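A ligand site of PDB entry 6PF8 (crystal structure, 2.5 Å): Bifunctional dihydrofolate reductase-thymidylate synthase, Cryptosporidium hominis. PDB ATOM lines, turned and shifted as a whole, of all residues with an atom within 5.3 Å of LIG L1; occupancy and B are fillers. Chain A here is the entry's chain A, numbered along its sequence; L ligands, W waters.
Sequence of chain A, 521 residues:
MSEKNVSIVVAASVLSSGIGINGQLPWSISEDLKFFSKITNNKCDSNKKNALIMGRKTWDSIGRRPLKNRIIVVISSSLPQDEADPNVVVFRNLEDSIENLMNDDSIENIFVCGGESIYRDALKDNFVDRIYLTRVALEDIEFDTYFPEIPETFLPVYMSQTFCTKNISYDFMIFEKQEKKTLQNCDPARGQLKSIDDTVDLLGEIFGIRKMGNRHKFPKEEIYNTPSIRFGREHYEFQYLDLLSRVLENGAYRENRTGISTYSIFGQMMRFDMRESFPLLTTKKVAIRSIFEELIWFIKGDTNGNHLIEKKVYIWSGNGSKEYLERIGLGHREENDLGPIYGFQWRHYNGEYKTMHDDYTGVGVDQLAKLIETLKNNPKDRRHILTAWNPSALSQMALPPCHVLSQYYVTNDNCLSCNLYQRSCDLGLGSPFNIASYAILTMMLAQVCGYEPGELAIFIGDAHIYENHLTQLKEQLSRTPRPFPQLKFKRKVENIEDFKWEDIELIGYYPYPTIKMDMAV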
ATOM      1  N   VAL A   9      -8.991 -10.486 -10.614  1.00  0.00           N
ATOM      2  CA  VAL A   9     -10.353  -9.972 -10.790  1.00  0.00           C
ATOM      3  C   VAL A   9     -10.484  -9.548 -12.242  1.00  0.00           C
ATOM      4  O   VAL A   9      -9.672  -8.765 -12.745  1.00  0.00           O
ATOM      5  CB  VAL A   9     -10.642  -8.792  -9.846  1.00  0.00           C
ATOM      6  CG1 VAL A   9     -12.127  -8.462  -9.853  1.00  0.00           C
ATOM      7  CG2 VAL A   9     -10.175  -9.095  -8.433  1.00  0.00           C
ATOM      8  N   VAL A  10     -11.517 -10.055 -12.915  1.00  0.00           N
ATOM      9  CA  VAL A  10     -11.694  -9.807 -14.339  1.00  0.00           C
ATOM     10  C   VAL A  10     -13.175  -9.947 -14.674  1.00  0.00           C
ATOM     11  O   VAL A  10     -13.897 -10.715 -14.040  1.00  0.00           O
ATOM     12  CB  VAL A  10     -10.824 -10.763 -15.186  1.00  0.00           C
ATOM     13  CG1 VAL A  10     -11.250 -12.208 -14.977  1.00  0.00           C
ATOM     14  CG2 VAL A  10     -10.866 -10.388 -16.666  1.00  0.00           C
ATOM     15  N   ALA A  11     -13.622  -9.191 -15.679  1.00  0.00           N
ATOM     16  CA  ALA A  11     -14.943  -9.343 -16.265  1.00  0.00           C
ATOM     17  C   ALA A  11     -14.761  -9.639 -17.750  1.00  0.00           C
ATOM     18  O   ALA A  11     -14.196  -8.822 -18.478  1.00  0.00           O
ATOM     19  CB  ALA A  11     -15.813  -8.103 -16.060  1.00  0.00           C
ATOM     20  N   LEU A  25     -13.773  -0.484 -21.853  1.00  0.00           N
ATOM     21  CA  LEU A  25     -14.558  -1.695 -21.695  1.00  0.00           C
ATOM     22  C   LEU A  25     -15.617  -1.787 -22.801  1.00  0.00           C
ATOM     23  O   LEU A  25     -16.106  -0.755 -23.278  1.00  0.00           O
ATOM     24  CB  LEU A  25     -15.237  -1.723 -20.331  1.00  0.00           C
ATOM     25  CG  LEU A  25     -14.336  -1.626 -19.105  1.00  0.00           C
ATOM     26  CD1 LEU A  25     -15.177  -1.632 -17.842  1.00  0.00           C
ATOM     27  CD2 LEU A  25     -13.314  -2.740 -19.094  1.00  0.00           C
ATOM     28  N   SER A  30     -22.841  -1.162 -13.915  1.00  0.00           N
ATOM     29  CA  SER A  30     -22.535  -0.490 -12.649  1.00  0.00           C
ATOM     30  C   SER A  30     -22.312  -1.490 -11.526  1.00  0.00           C
ATOM     31  O   SER A  30     -21.386  -1.331 -10.719  1.00  0.00           O
ATOM     32  CB  SER A  30     -23.663   0.479 -12.303  1.00  0.00           C
ATOM     33  OG  SER A  30     -23.502   0.996 -10.997  1.00  0.00           O
ATOM     34  N   ASP A  32     -21.133  -4.390 -11.576  1.00  0.00           N
ATOM     35  CA  ASP A  32     -19.851  -5.082 -11.669  1.00  0.00           C
ATOM     36  C   ASP A  32     -18.712  -4.239 -11.105  1.00  0.00           C
ATOM     37  O   ASP A  32     -17.775  -4.771 -10.499  1.00  0.00           O
ATOM     38  CB  ASP A  32     -19.559  -5.467 -13.121  1.00  0.00           C
ATOM     39  CG  ASP A  32     -18.192  -6.078 -13.295  1.00  0.00           C
ATOM     40  OD1 ASP A  32     -17.925  -7.147 -12.690  1.00  0.00           O
ATOM     41  OD2 ASP A  32     -17.385  -5.492 -14.042  1.00  0.00           O
ATOM     42  N   LEU A  33     -18.777  -2.918 -11.285  1.00  0.00           N
ATOM     43  CA  LEU A  33     -17.774  -2.040 -10.687  1.00  0.00           C
ATOM     44  C   LEU A  33     -17.890  -2.039  -9.167  1.00  0.00           C
ATOM     45  O   LEU A  33     -16.881  -1.983  -8.464  1.00  0.00           O
ATOM     46  CB  LEU A  33     -17.899  -0.626 -11.236  1.00  0.00           C
ATOM     47  CG  LEU A  33     -17.539  -0.438 -12.718  1.00  0.00           C
ATOM     48  CD1 LEU A  33     -17.566   1.036 -13.096  1.00  0.00           C
ATOM     49  CD2 LEU A  33     -16.186  -1.063 -13.036  1.00  0.00           C
ATOM     50  N   LYS A  34     -19.119  -2.096  -8.650  1.00  0.00           N
ATOM     51  CA  LYS A  34     -19.298  -2.198  -7.202  1.00  0.00           C
ATOM     52  C   LYS A  34     -18.728  -3.502  -6.676  1.00  0.00           C
ATOM     53  O   LYS A  34     -18.140  -3.537  -5.590  1.00  0.00           O
ATOM     54  CB  LYS A  34     -20.780  -2.075  -6.846  1.00  0.00           C
ATOM     55  CG  LYS A  34     -21.408  -0.760  -7.289  1.00  0.00           C
ATOM     56  CD  LYS A  34     -22.783  -0.574  -6.696  1.00  0.00           C
ATOM     57  CE  LYS A  34     -23.461   0.670  -7.258  1.00  0.00           C
ATOM     58  NZ  LYS A  34     -22.595   1.876  -7.136  1.00  0.00           N
ATOM     59  N   PHE A  35     -18.868  -4.585  -7.444  1.00  0.00           N
ATOM     60  CA  PHE A  35     -18.248  -5.854  -7.056  1.00  0.00           C
ATOM     61  C   PHE A  35     -16.730  -5.730  -7.038  1.00  0.00           C
ATOM     62  O   PHE A  35     -16.070  -6.168  -6.089  1.00  0.00           O
ATOM     63  CB  PHE A  35     -18.701  -6.971  -7.992  1.00  0.00           C
ATOM     64  CG  PHE A  35     -18.076  -8.307  -7.687  1.00  0.00           C
ATOM     65  CD1 PHE A  35     -18.525  -9.062  -6.611  1.00  0.00           C
ATOM     66  CD2 PHE A  35     -17.055  -8.805  -8.466  1.00  0.00           C
ATOM     67  CE1 PHE A  35     -17.952 -10.294  -6.326  1.00  0.00           C
ATOM     68  CE2 PHE A  35     -16.481 -10.030  -8.194  1.00  0.00           C
ATOM     69  CZ  PHE A  35     -16.930 -10.785  -7.118  1.00  0.00           C
ATOM     70  N   PHE A  36     -16.153  -5.142  -8.090  1.00  0.00           N
ATOM     71  CA  PHE A  36     -14.710  -4.906  -8.090  1.00  0.00           C
ATOM     72  C   PHE A  36     -14.287  -4.094  -6.882  1.00  0.00           C
ATOM     73  O   PHE A  36     -13.257  -4.389  -6.253  1.00  0.00           O
ATOM     74  CB  PHE A  36     -14.282  -4.220  -9.386  1.00  0.00           C
ATOM     75  CG  PHE A  36     -12.828  -3.851  -9.413  1.00  0.00           C
ATOM     76  CD1 PHE A  36     -11.875  -4.755  -9.831  1.00  0.00           C
ATOM     77  CD2 PHE A  36     -12.413  -2.586  -9.015  1.00  0.00           C
ATOM     78  CE1 PHE A  36     -10.537  -4.422  -9.843  1.00  0.00           C
ATOM     79  CE2 PHE A  36     -11.081  -2.246  -9.024  1.00  0.00           C
ATOM     80  CZ  PHE A  36     -10.135  -3.157  -9.438  1.00  0.00           C
ATOM     81  N   SER A  37     -15.052  -3.065  -6.541  1.00  0.00           N
ATOM     82  CA  SER A  37     -14.700  -2.228  -5.395  1.00  0.00           C
ATOM     83  C   SER A  37     -14.792  -2.996  -4.091  1.00  0.00           C
ATOM     84  O   SER A  37     -13.891  -2.905  -3.241  1.00  0.00           O
ATOM     85  CB  SER A  37     -15.599  -0.990  -5.360  1.00  0.00           C
ATOM     86  OG  SER A  37     -15.280  -0.163  -4.253  1.00  0.00           O
ATOM     87  N   THR A  40     -11.971  -5.816  -3.773  1.00  0.00           N
ATOM     88  CA  THR A  40     -10.599  -5.339  -3.614  1.00  0.00           C
ATOM     89  C   THR A  40     -10.395  -4.539  -2.328  1.00  0.00           C
ATOM     90  O   THR A  40      -9.243  -4.369  -1.909  1.00  0.00           O
ATOM     91  CB  THR A  40     -10.168  -4.484  -4.816  1.00  0.00           C
ATOM     92  OG1 THR A  40     -11.058  -3.377  -4.990  1.00  0.00           O
ATOM     93  CG2 THR A  40     -10.147  -5.317  -6.098  1.00  0.00           C
ATOM     94  N   ASN A  41     -11.464  -4.051  -1.708  1.00  0.00           N
ATOM     95  CA  ASN A  41     -11.367  -3.386  -0.417  1.00  0.00           C
ATOM     96  C   ASN A  41     -11.490  -4.345   0.764  1.00  0.00           C
ATOM     97  O   ASN A  41     -11.125  -3.962   1.893  1.00  0.00           O
ATOM     98  CB  ASN A  41     -12.455  -2.308  -0.291  1.00  0.00           C
ATOM     99  CG  ASN A  41     -12.037  -0.984  -0.912  1.00  0.00           C
ATOM    100  OD1 ASN A  41     -10.968  -0.461  -0.627  1.00  0.00           O
ATOM    101  ND2 ASN A  41     -12.901  -0.430  -1.765  1.00  0.00           N
ATOM    102  N   THR A  58      -4.176  -0.057 -18.740  1.00  0.00           N
ATOM    103  CA  THR A  58      -5.303  -0.020 -17.821  1.00  0.00           C
ATOM    104  C   THR A  58      -5.199   1.171 -16.873  1.00  0.00           C
ATOM    105  O   THR A  58      -6.218   1.793 -16.539  1.00  0.00           O
ATOM    106  CB  THR A  58      -5.384  -1.340 -17.044  1.00  0.00           C
ATOM    107  OG1 THR A  58      -5.567  -2.417 -17.962  1.00  0.00           O
ATOM    108  CG2 THR A  58      -6.538  -1.315 -16.061  1.00  0.00           C
ATOM    109  N   SER A  61      -6.600   3.953 -18.740  1.00  0.00           N
ATOM    110  CA  SER A  61      -8.038   3.890 -18.953  1.00  0.00           C
ATOM    111  C   SER A  61      -8.848   4.321 -17.736  1.00  0.00           C
ATOM    112  O   SER A  61     -10.007   4.711 -17.877  1.00  0.00           O
ATOM    113  CB  SER A  61      -8.455   2.476 -19.364  1.00  0.00           C
ATOM    114  OG  SER A  61      -8.276   1.564 -18.301  1.00  0.00           O
ATOM    115  N   ILE A  62      -8.273   4.249 -16.533  1.00  0.00           N
ATOM    116  CA  ILE A  62      -8.983   4.674 -15.330  1.00  0.00           C
ATOM    117  C   ILE A  62      -8.608   6.112 -14.988  1.00  0.00           C
ATOM    118  O   ILE A  62      -8.846   6.587 -13.869  1.00  0.00           O
ATOM    119  CB  ILE A  62      -8.707   3.741 -14.137  1.00  0.00           C
ATOM    120  CG1 ILE A  62      -7.228   3.771 -13.748  1.00  0.00           C
ATOM    121  CG2 ILE A  62      -9.152   2.324 -14.472  1.00  0.00           C
ATOM    122  CD1 ILE A  62      -6.921   2.947 -12.523  1.00  0.00           C
ATOM    123  N   LEU A  67      -7.278   4.861  -6.399  1.00  0.00           N
ATOM    124  CA  LEU A  67      -8.487   4.231  -5.871  1.00  0.00           C
ATOM    125  C   LEU A  67      -8.477   4.326  -4.352  1.00  0.00           C
ATOM    126  O   LEU A  67      -7.499   3.939  -3.710  1.00  0.00           O
ATOM    127  CB  LEU A  67      -8.571   2.769  -6.320  1.00  0.00           C
ATOM    128  CG  LEU A  67      -8.801   2.560  -7.815  1.00  0.00           C
ATOM    129  CD1 LEU A  67      -8.675   1.104  -8.193  1.00  0.00           C
ATOM    130  CD2 LEU A  67     -10.167   3.098  -8.202  1.00  0.00           C
ATOM    131  N   ARG A  70      -6.831   2.017  -1.229  1.00  0.00           N
ATOM    132  CA  ARG A  70      -5.999   0.976  -1.811  1.00  0.00           C
ATOM    133  C   ARG A  70      -4.745   1.581  -2.412  1.00  0.00           C
ATOM    134  O   ARG A  70      -4.649   2.787  -2.649  1.00  0.00           O
ATOM    135  CB  ARG A  70      -6.768   0.175  -2.866  1.00  0.00           C
ATOM    136  CG  ARG A  70      -7.796  -0.783  -2.290  1.00  0.00           C
ATOM    137  CD  ARG A  70      -8.955  -0.960  -3.245  1.00  0.00           C
ATOM    138  NE  ARG A  70      -9.717   0.278  -3.378  1.00  0.00           N
ATOM    139  CZ  ARG A  70     -10.707   0.461  -4.260  1.00  0.00           C
ATOM    140  NH1 ARG A  70     -11.060  -0.520  -5.066  1.00  0.00           N
ATOM    141  NH2 ARG A  70     -11.340   1.627  -4.303  1.00  0.00           N
ATOM    142  N   VAL A 112      -4.491  -8.933  -8.982  1.00  0.00           N
ATOM    143  CA  VAL A 112      -4.109  -8.684 -10.376  1.00  0.00           C
ATOM    144  C   VAL A 112      -5.369  -8.176 -11.075  1.00  0.00           C
ATOM    145  O   VAL A 112      -6.324  -8.926 -11.263  1.00  0.00           O
ATOM    146  CB  VAL A 112      -3.552  -9.946 -11.045  1.00  0.00           C
ATOM    147  CG1 VAL A 112      -3.218  -9.665 -12.506  1.00  0.00           C
ATOM    148  CG2 VAL A 112      -2.324 -10.431 -10.305  1.00  0.00           C
ATOM    149  N   CYS A 113      -5.364  -6.900 -11.448  1.00  0.00           N
ATOM    150  CA  CYS A 113      -6.602  -6.184 -11.714  1.00  0.00           C
ATOM    151  C   CYS A 113      -6.869  -5.896 -13.179  1.00  0.00           C
ATOM    152  O   CYS A 113      -7.934  -5.344 -13.495  1.00  0.00           O
ATOM    153  CB  CYS A 113      -6.622  -4.862 -10.945  1.00  0.00           C
ATOM    154  SG  CYS A 113      -6.963  -5.085  -9.201  1.00  0.00           S
ATOM    155  N   GLY A 114      -5.975  -6.232 -14.089  1.00  0.00           N
ATOM    156  CA  GLY A 114      -6.345  -6.040 -15.474  1.00  0.00           C
ATOM    157  C   GLY A 114      -5.180  -5.829 -16.408  1.00  0.00           C
ATOM    158  O   GLY A 114      -4.069  -5.477 -16.009  1.00  0.00           O
ATOM    159  N   TYR A 119      -2.525 -10.239 -17.069  1.00  0.00           N
ATOM    160  CA  TYR A 119      -3.213 -11.499 -16.780  1.00  0.00           C
ATOM    161  C   TYR A 119      -2.406 -12.686 -17.302  1.00  0.00           C
ATOM    162  O   TYR A 119      -2.204 -13.680 -16.591  1.00  0.00           O
ATOM    163  CB  TYR A 119      -4.603 -11.512 -17.402  1.00  0.00           C
ATOM    164  CG  TYR A 119      -5.646 -10.666 -16.725  1.00  0.00           C
ATOM    165  CD1 TYR A 119      -5.704 -10.551 -15.342  1.00  0.00           C
ATOM    166  CD2 TYR A 119      -6.599  -9.987 -17.470  1.00  0.00           C
ATOM    167  CE1 TYR A 119      -6.672  -9.779 -14.729  1.00  0.00           C
ATOM    168  CE2 TYR A 119      -7.567  -9.208 -16.871  1.00  0.00           C
ATOM    169  CZ  TYR A 119      -7.606  -9.115 -15.498  1.00  0.00           C
ATOM    170  OH  TYR A 119      -8.573  -8.329 -14.911  1.00  0.00           O
ATOM    171  N   THR A 134     -16.301 -12.352 -13.702  1.00  0.00           N
ATOM    172  CA  THR A 134     -17.646 -11.897 -14.051  1.00  0.00           C
ATOM    173  C   THR A 134     -17.880 -12.261 -15.521  1.00  0.00           C
ATOM    174  O   THR A 134     -17.232 -11.713 -16.414  1.00  0.00           O
ATOM    175  CB  THR A 134     -17.796 -10.386 -13.836  1.00  0.00           C
ATOM    176  OG1 THR A 134     -17.444 -10.056 -12.496  1.00  0.00           O
ATOM    177  CG2 THR A 134     -19.239  -9.976 -14.086  1.00  0.00           C
HETATM  178  N1  LIG L   1     -14.625  -5.666 -13.632  1.00  0.00           N
HETATM  179  C1  LIG L   1     -14.278  -6.805 -13.002  1.00  0.00           C
HETATM  180  N2  LIG L   1     -15.306  -7.730 -12.616  1.00  0.00           N
HETATM  181  N3  LIG L   1     -13.002  -7.100 -12.703  1.00  0.00           N
HETATM  182  C2  LIG L   1     -12.004  -6.250 -13.041  1.00  0.00           C
HETATM  183  N4  LIG L   1     -10.641  -6.524 -12.750  1.00  0.00           N
HETATM  184  C3  LIG L   1     -12.327  -5.057 -13.714  1.00  0.00           C
HETATM  185  N5  LIG L   1     -11.340  -4.187 -14.058  1.00  0.00           N
HETATM  186  C4  LIG L   1     -11.670  -3.056 -14.699  1.00  0.00           C
HETATM  187  C5  LIG L   1     -13.003  -2.747 -15.011  1.00  0.00           C
HETATM  188  N6  LIG L   1     -13.974  -3.616 -14.641  1.00  0.00           N
HETATM  189  C6  LIG L   1     -13.650  -4.782 -13.994  1.00  0.00           C
HETATM  190  C7  LIG L   1     -10.568  -2.100 -15.074  1.00  0.00           C
HETATM  191  N7  LIG L   1     -11.013  -0.734 -15.115  1.00  0.00           N
HETATM  192  C8  LIG L   1     -10.975  -0.021 -16.371  1.00  0.00           C
HETATM  193  C9  LIG L   1     -12.628   1.137 -11.672  1.00  0.00           C
HETATM  194  C10 LIG L   1     -13.138   1.390 -12.938  1.00  0.00           C
HETATM  195  C11 LIG L   1     -12.586   0.778 -14.055  1.00  0.00           C
HETATM  196  C12 LIG L   1     -11.535  -0.109 -13.911  1.00  0.00           C
HETATM  197  C13 LIG L   1     -11.019  -0.390 -12.635  1.00  0.00           C
HETATM  198  C14 LIG L   1     -11.571   0.237 -11.519  1.00  0.00           C
HETATM  199  C15 LIG L   1     -13.270   1.830 -10.503  1.00  0.00           C
HETATM  200  O1  LIG L   1     -13.796   2.912 -10.679  1.00  0.00           O
HETATM  201  N8  LIG L   1     -13.332   1.247  -9.182  1.00  0.00           N
HETATM  202  C16 LIG L   1     -13.985   1.969  -8.126  1.00  0.00           C
HETATM  203  C17 LIG L   1     -13.490   1.455  -6.836  1.00  0.00           C
HETATM  204  O2  LIG L   1     -12.822   0.387  -6.820  1.00  0.00           O
HETATM  205  O3  LIG L   1     -13.721   2.083  -5.765  1.00  0.00           O
HETATM  206  C18 LIG L   1     -15.438   1.629  -8.219  1.00  0.00           C
HETATM  207  C19 LIG L   1     -16.486   2.680  -8.081  1.00  0.00           C
HETATM  208  C20 LIG L   1     -17.892   2.168  -7.957  1.00  0.00           C
HETATM  209  O4  LIG L   1     -18.351   1.905  -6.821  1.00  0.00           O
HETATM  210  O5  LIG L   1     -18.671   2.256  -8.940  1.00  0.00           O
HETATM  211  P1  LG2 L   2      -2.298  -3.544 -20.260  1.00  0.00           P
HETATM  212  O1  LG2 L   2      -1.888  -4.970 -20.004  1.00  0.00           O
HETATM  213  O2  LG2 L   2      -3.292  -3.097 -19.235  1.00  0.00           O
HETATM  214  O3  LG2 L   2      -1.074  -2.632 -20.142  1.00  0.00           O
HETATM  215  C1  LG2 L   2       0.070  -2.893 -20.905  1.00  0.00           C
HETATM  216  C2  LG2 L   2       1.291  -2.165 -20.515  1.00  0.00           C
HETATM  217  O4  LG2 L   2       1.796  -2.690 -19.301  1.00  0.00           O
HETATM  218  C3  LG2 L   2       2.387  -2.323 -21.466  1.00  0.00           C
HETATM  219  O5  LG2 L   2       2.279  -1.454 -22.547  1.00  0.00           O
HETATM  220  C4  LG2 L   2       3.530  -1.998 -20.651  1.00  0.00           C
HETATM  221  O6  LG2 L   2       3.605  -0.618 -20.403  1.00  0.00           O
HETATM  222  C5  LG2 L   2       3.213  -2.658 -19.391  1.00  0.00           C
HETATM  223  N1  LG2 L   2       3.735  -3.969 -19.388  1.00  0.00           N
HETATM  224  C6  LG2 L   2       3.063  -5.103 -19.669  1.00  0.00           C
HETATM  225  N2  LG2 L   2       3.898  -6.157 -19.558  1.00  0.00           N
HETATM  226  C7  LG2 L   2       5.137  -5.692 -19.199  1.00  0.00           C
HETATM  227  C8  LG2 L   2       6.390  -6.295 -18.938  1.00  0.00           C
HETATM  228  N3  LG2 L   2       6.522  -7.772 -19.049  1.00  0.00           N
HETATM  229  N4  LG2 L   2       7.457  -5.528 -18.584  1.00  0.00           N
HETATM  230  C9  LG2 L   2       7.310  -4.179 -18.491  1.00  0.00           C
HETATM  231  N5  LG2 L   2       6.141  -3.560 -18.723  1.00  0.00           N
HETATM  232  C10 LG2 L   2       5.035  -4.300 -19.089  1.00  0.00           C
HETATM  233  O7  LG2 L   2      -2.916  -3.359 -21.725  1.00  0.00           O
HETATM  234  P2  LG2 L   2      -4.016  -4.310 -22.342  1.00  0.00           P
HETATM  235  O8  LG2 L   2      -4.284  -3.938 -23.811  1.00  0.00           O
HETATM  236  O9  LG2 L   2      -3.545  -5.756 -22.323  1.00  0.00           O
HETATM  237  O10 LG2 L   2      -5.368  -4.152 -21.467  1.00  0.00           O
HETATM  238  C11 LG2 L   2      -6.169  -3.006 -21.593  1.00  0.00           C
HETATM  239  C12 LG2 L   2      -7.516  -3.205 -22.125  1.00  0.00           C
HETATM  240  O11 LG2 L   2      -8.178  -4.227 -21.372  1.00  0.00           O
HETATM  241  C13 LG2 L   2      -8.318  -1.981 -21.973  1.00  0.00           C
HETATM  242  O12 LG2 L   2      -9.269  -1.925 -22.989  1.00  0.00           O
HETATM  243  C14 LG2 L   2      -8.965  -2.169 -20.713  1.00  0.00           C
HETATM  244  O13 LG2 L   2     -10.132  -1.413 -20.637  1.00  0.00           O
HETATM  245  C15 LG2 L   2      -9.251  -3.617 -20.721  1.00  0.00           C
HETATM  246  N6  LG2 L   2      -9.401  -4.100 -19.386  1.00  0.00           N
HETATM  247  C16 LG2 L   2     -10.460  -4.883 -19.095  1.00  0.00           C
HETATM  248  C17 LG2 L   2     -10.648  -5.390 -17.807  1.00  0.00           C
HETATM  249  C18 LG2 L   2     -11.857  -6.259 -17.513  1.00  0.00           C
HETATM  250  O14 LG2 L   2     -11.921  -6.861 -16.424  1.00  0.00           O
HETATM  251  N7  LG2 L   2     -12.919  -6.413 -18.459  1.00  0.00           N
HETATM  252  C19 LG2 L   2      -9.719  -5.071 -16.799  1.00  0.00           C
HETATM  253  C20 LG2 L   2      -8.634  -4.263 -17.130  1.00  0.00           C
HETATM  254  C21 LG2 L   2      -8.481  -3.778 -18.432  1.00  0.00           C
HETATM  255  P3  LG2 L   2       4.663   0.292 -21.089  1.00  0.00           P
HETATM  256  O15 LG2 L   2       4.301   0.457 -22.582  1.00  0.00           O
HETATM  257  O16 LG2 L   2       4.674   1.609 -20.432  1.00  0.00           O
HETATM  258  O17 LG2 L   2       6.024  -0.309 -20.965  1.00  0.00           O
HETATM  259  O   HOH W   1     -17.845   2.583  -4.007  1.00  0.00           O
HETATM  260  O   HOH W   2     -14.935 -10.249 -11.187  1.00  0.00           O
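An oxygen (O3) of LIG L1 lies within hydrogen-bond range of the side-chain hydroxyl of Ser 37 (3.1 Å). An oxygen (O2) of LG2 L2 lies within hydrogen-bond range of the backbone NH of Thr 58 (3.2 Å). The backbone carbonyl oxygen (O) of Cys 113 sits at hydrogen-bond distance from a nitrogen (N4) of LIG L1 (3.0 Å). A nitrogen (N2) of LIG L1 lies within hydrogen-bond range of the side-chain hydroxyl (OG1) of Thr 134, at 3.2 Å. The side-chain hydroxyl (OG1) of Thr 58 lies within hydrogen-bond range of an oxygen (O2) of LG2 L2 (2.7 Å). OH of Tyr 119 lies within hydrogen-bond range of N4 of LIG L1 (3.5 Å). NH1 of Arg 70 lies within salt-bridge range of O2 of LIG L1, at 2.6 Å. The backbone carbonyl oxygen of Val 9 lies within hydrogen-bond range of a nitrogen (N4) of LIG L1, 2.4 Å away. A nitrogen (N2) of LIG L1 is in hydrogen-bond range of the side-chain carboxylate (OD1) of Asp 32 (2.7 Å). The backbone carbonyl oxygen of Ala 11 sits at hydrogen-bond distance from a nitrogen (N7) of LG2 L2 (2.7 Å). N of Val 10 lies within hydrogen-bond range of N3 of LIG L1, at 3.3 Å. The backbone NH (N) of Ala 11 is in hydrogen-bond range of an oxygen (O14) of LG2 L2, at 3.0 Å.
O of Val 112 sits at hydrogen-bond distance from N of Val 9 (3.2 Å). The backbone carbonyl oxygen of Thr 58 lies within hydrogen-bond range of the side-chain hydroxyl of Ser 61, at 2.7 Å. The backbone carbonyl oxygen of Val 9 is in hydrogen-bond range of the side-chain hydroxyl of Tyr 119 (2.5 Å). The side-chain carboxylate (OD1) of Asp 32 sits at hydrogen-bond distance from the side-chain hydroxyl (OG1) of Thr 134 (3.0 Å). The backbone carbonyl oxygen of Val 10 lies within hydrogen-bond range of the backbone NH of Thr 134 (2.9 Å). OG1 of Thr 40 sits at hydrogen-bond distance from O of Phe 36, at 2.7 Å. The backbone carbonyl oxygen (O) of Cys 113 is in hydrogen-bond range of the side-chain hydroxyl (OH) of Tyr 119 (3.4 Å). The guanidinium group of Arg 70 lies within hydrogen-bond range of the side-chain amide oxygen of Asn 41 (3.1 Å).
Residues that only touch LIG L1: Ala 11, Leu 25, Leu 33, Phe 36, Ser 61, Ile 62 and Leu 67. Hydrophobic or aromatic side chains within 4 Å of LIG L1: Val 9, Ala 11, Leu 25, Leu 33, Phe 36, Ile 62 and Leu 67. The nearest printed residue that does not touch LIG L1 is Lys 34 (4.1 Å).
Water W2 lies within hydrogen-bond range of the side-chain hydroxyl (OG1) of Thr 134 (2.8 Å), a nitrogen (N2) of LIG L1 (2.9 Å) and the backbone carbonyl oxygen (O) of Val 10 (3.1 Å).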
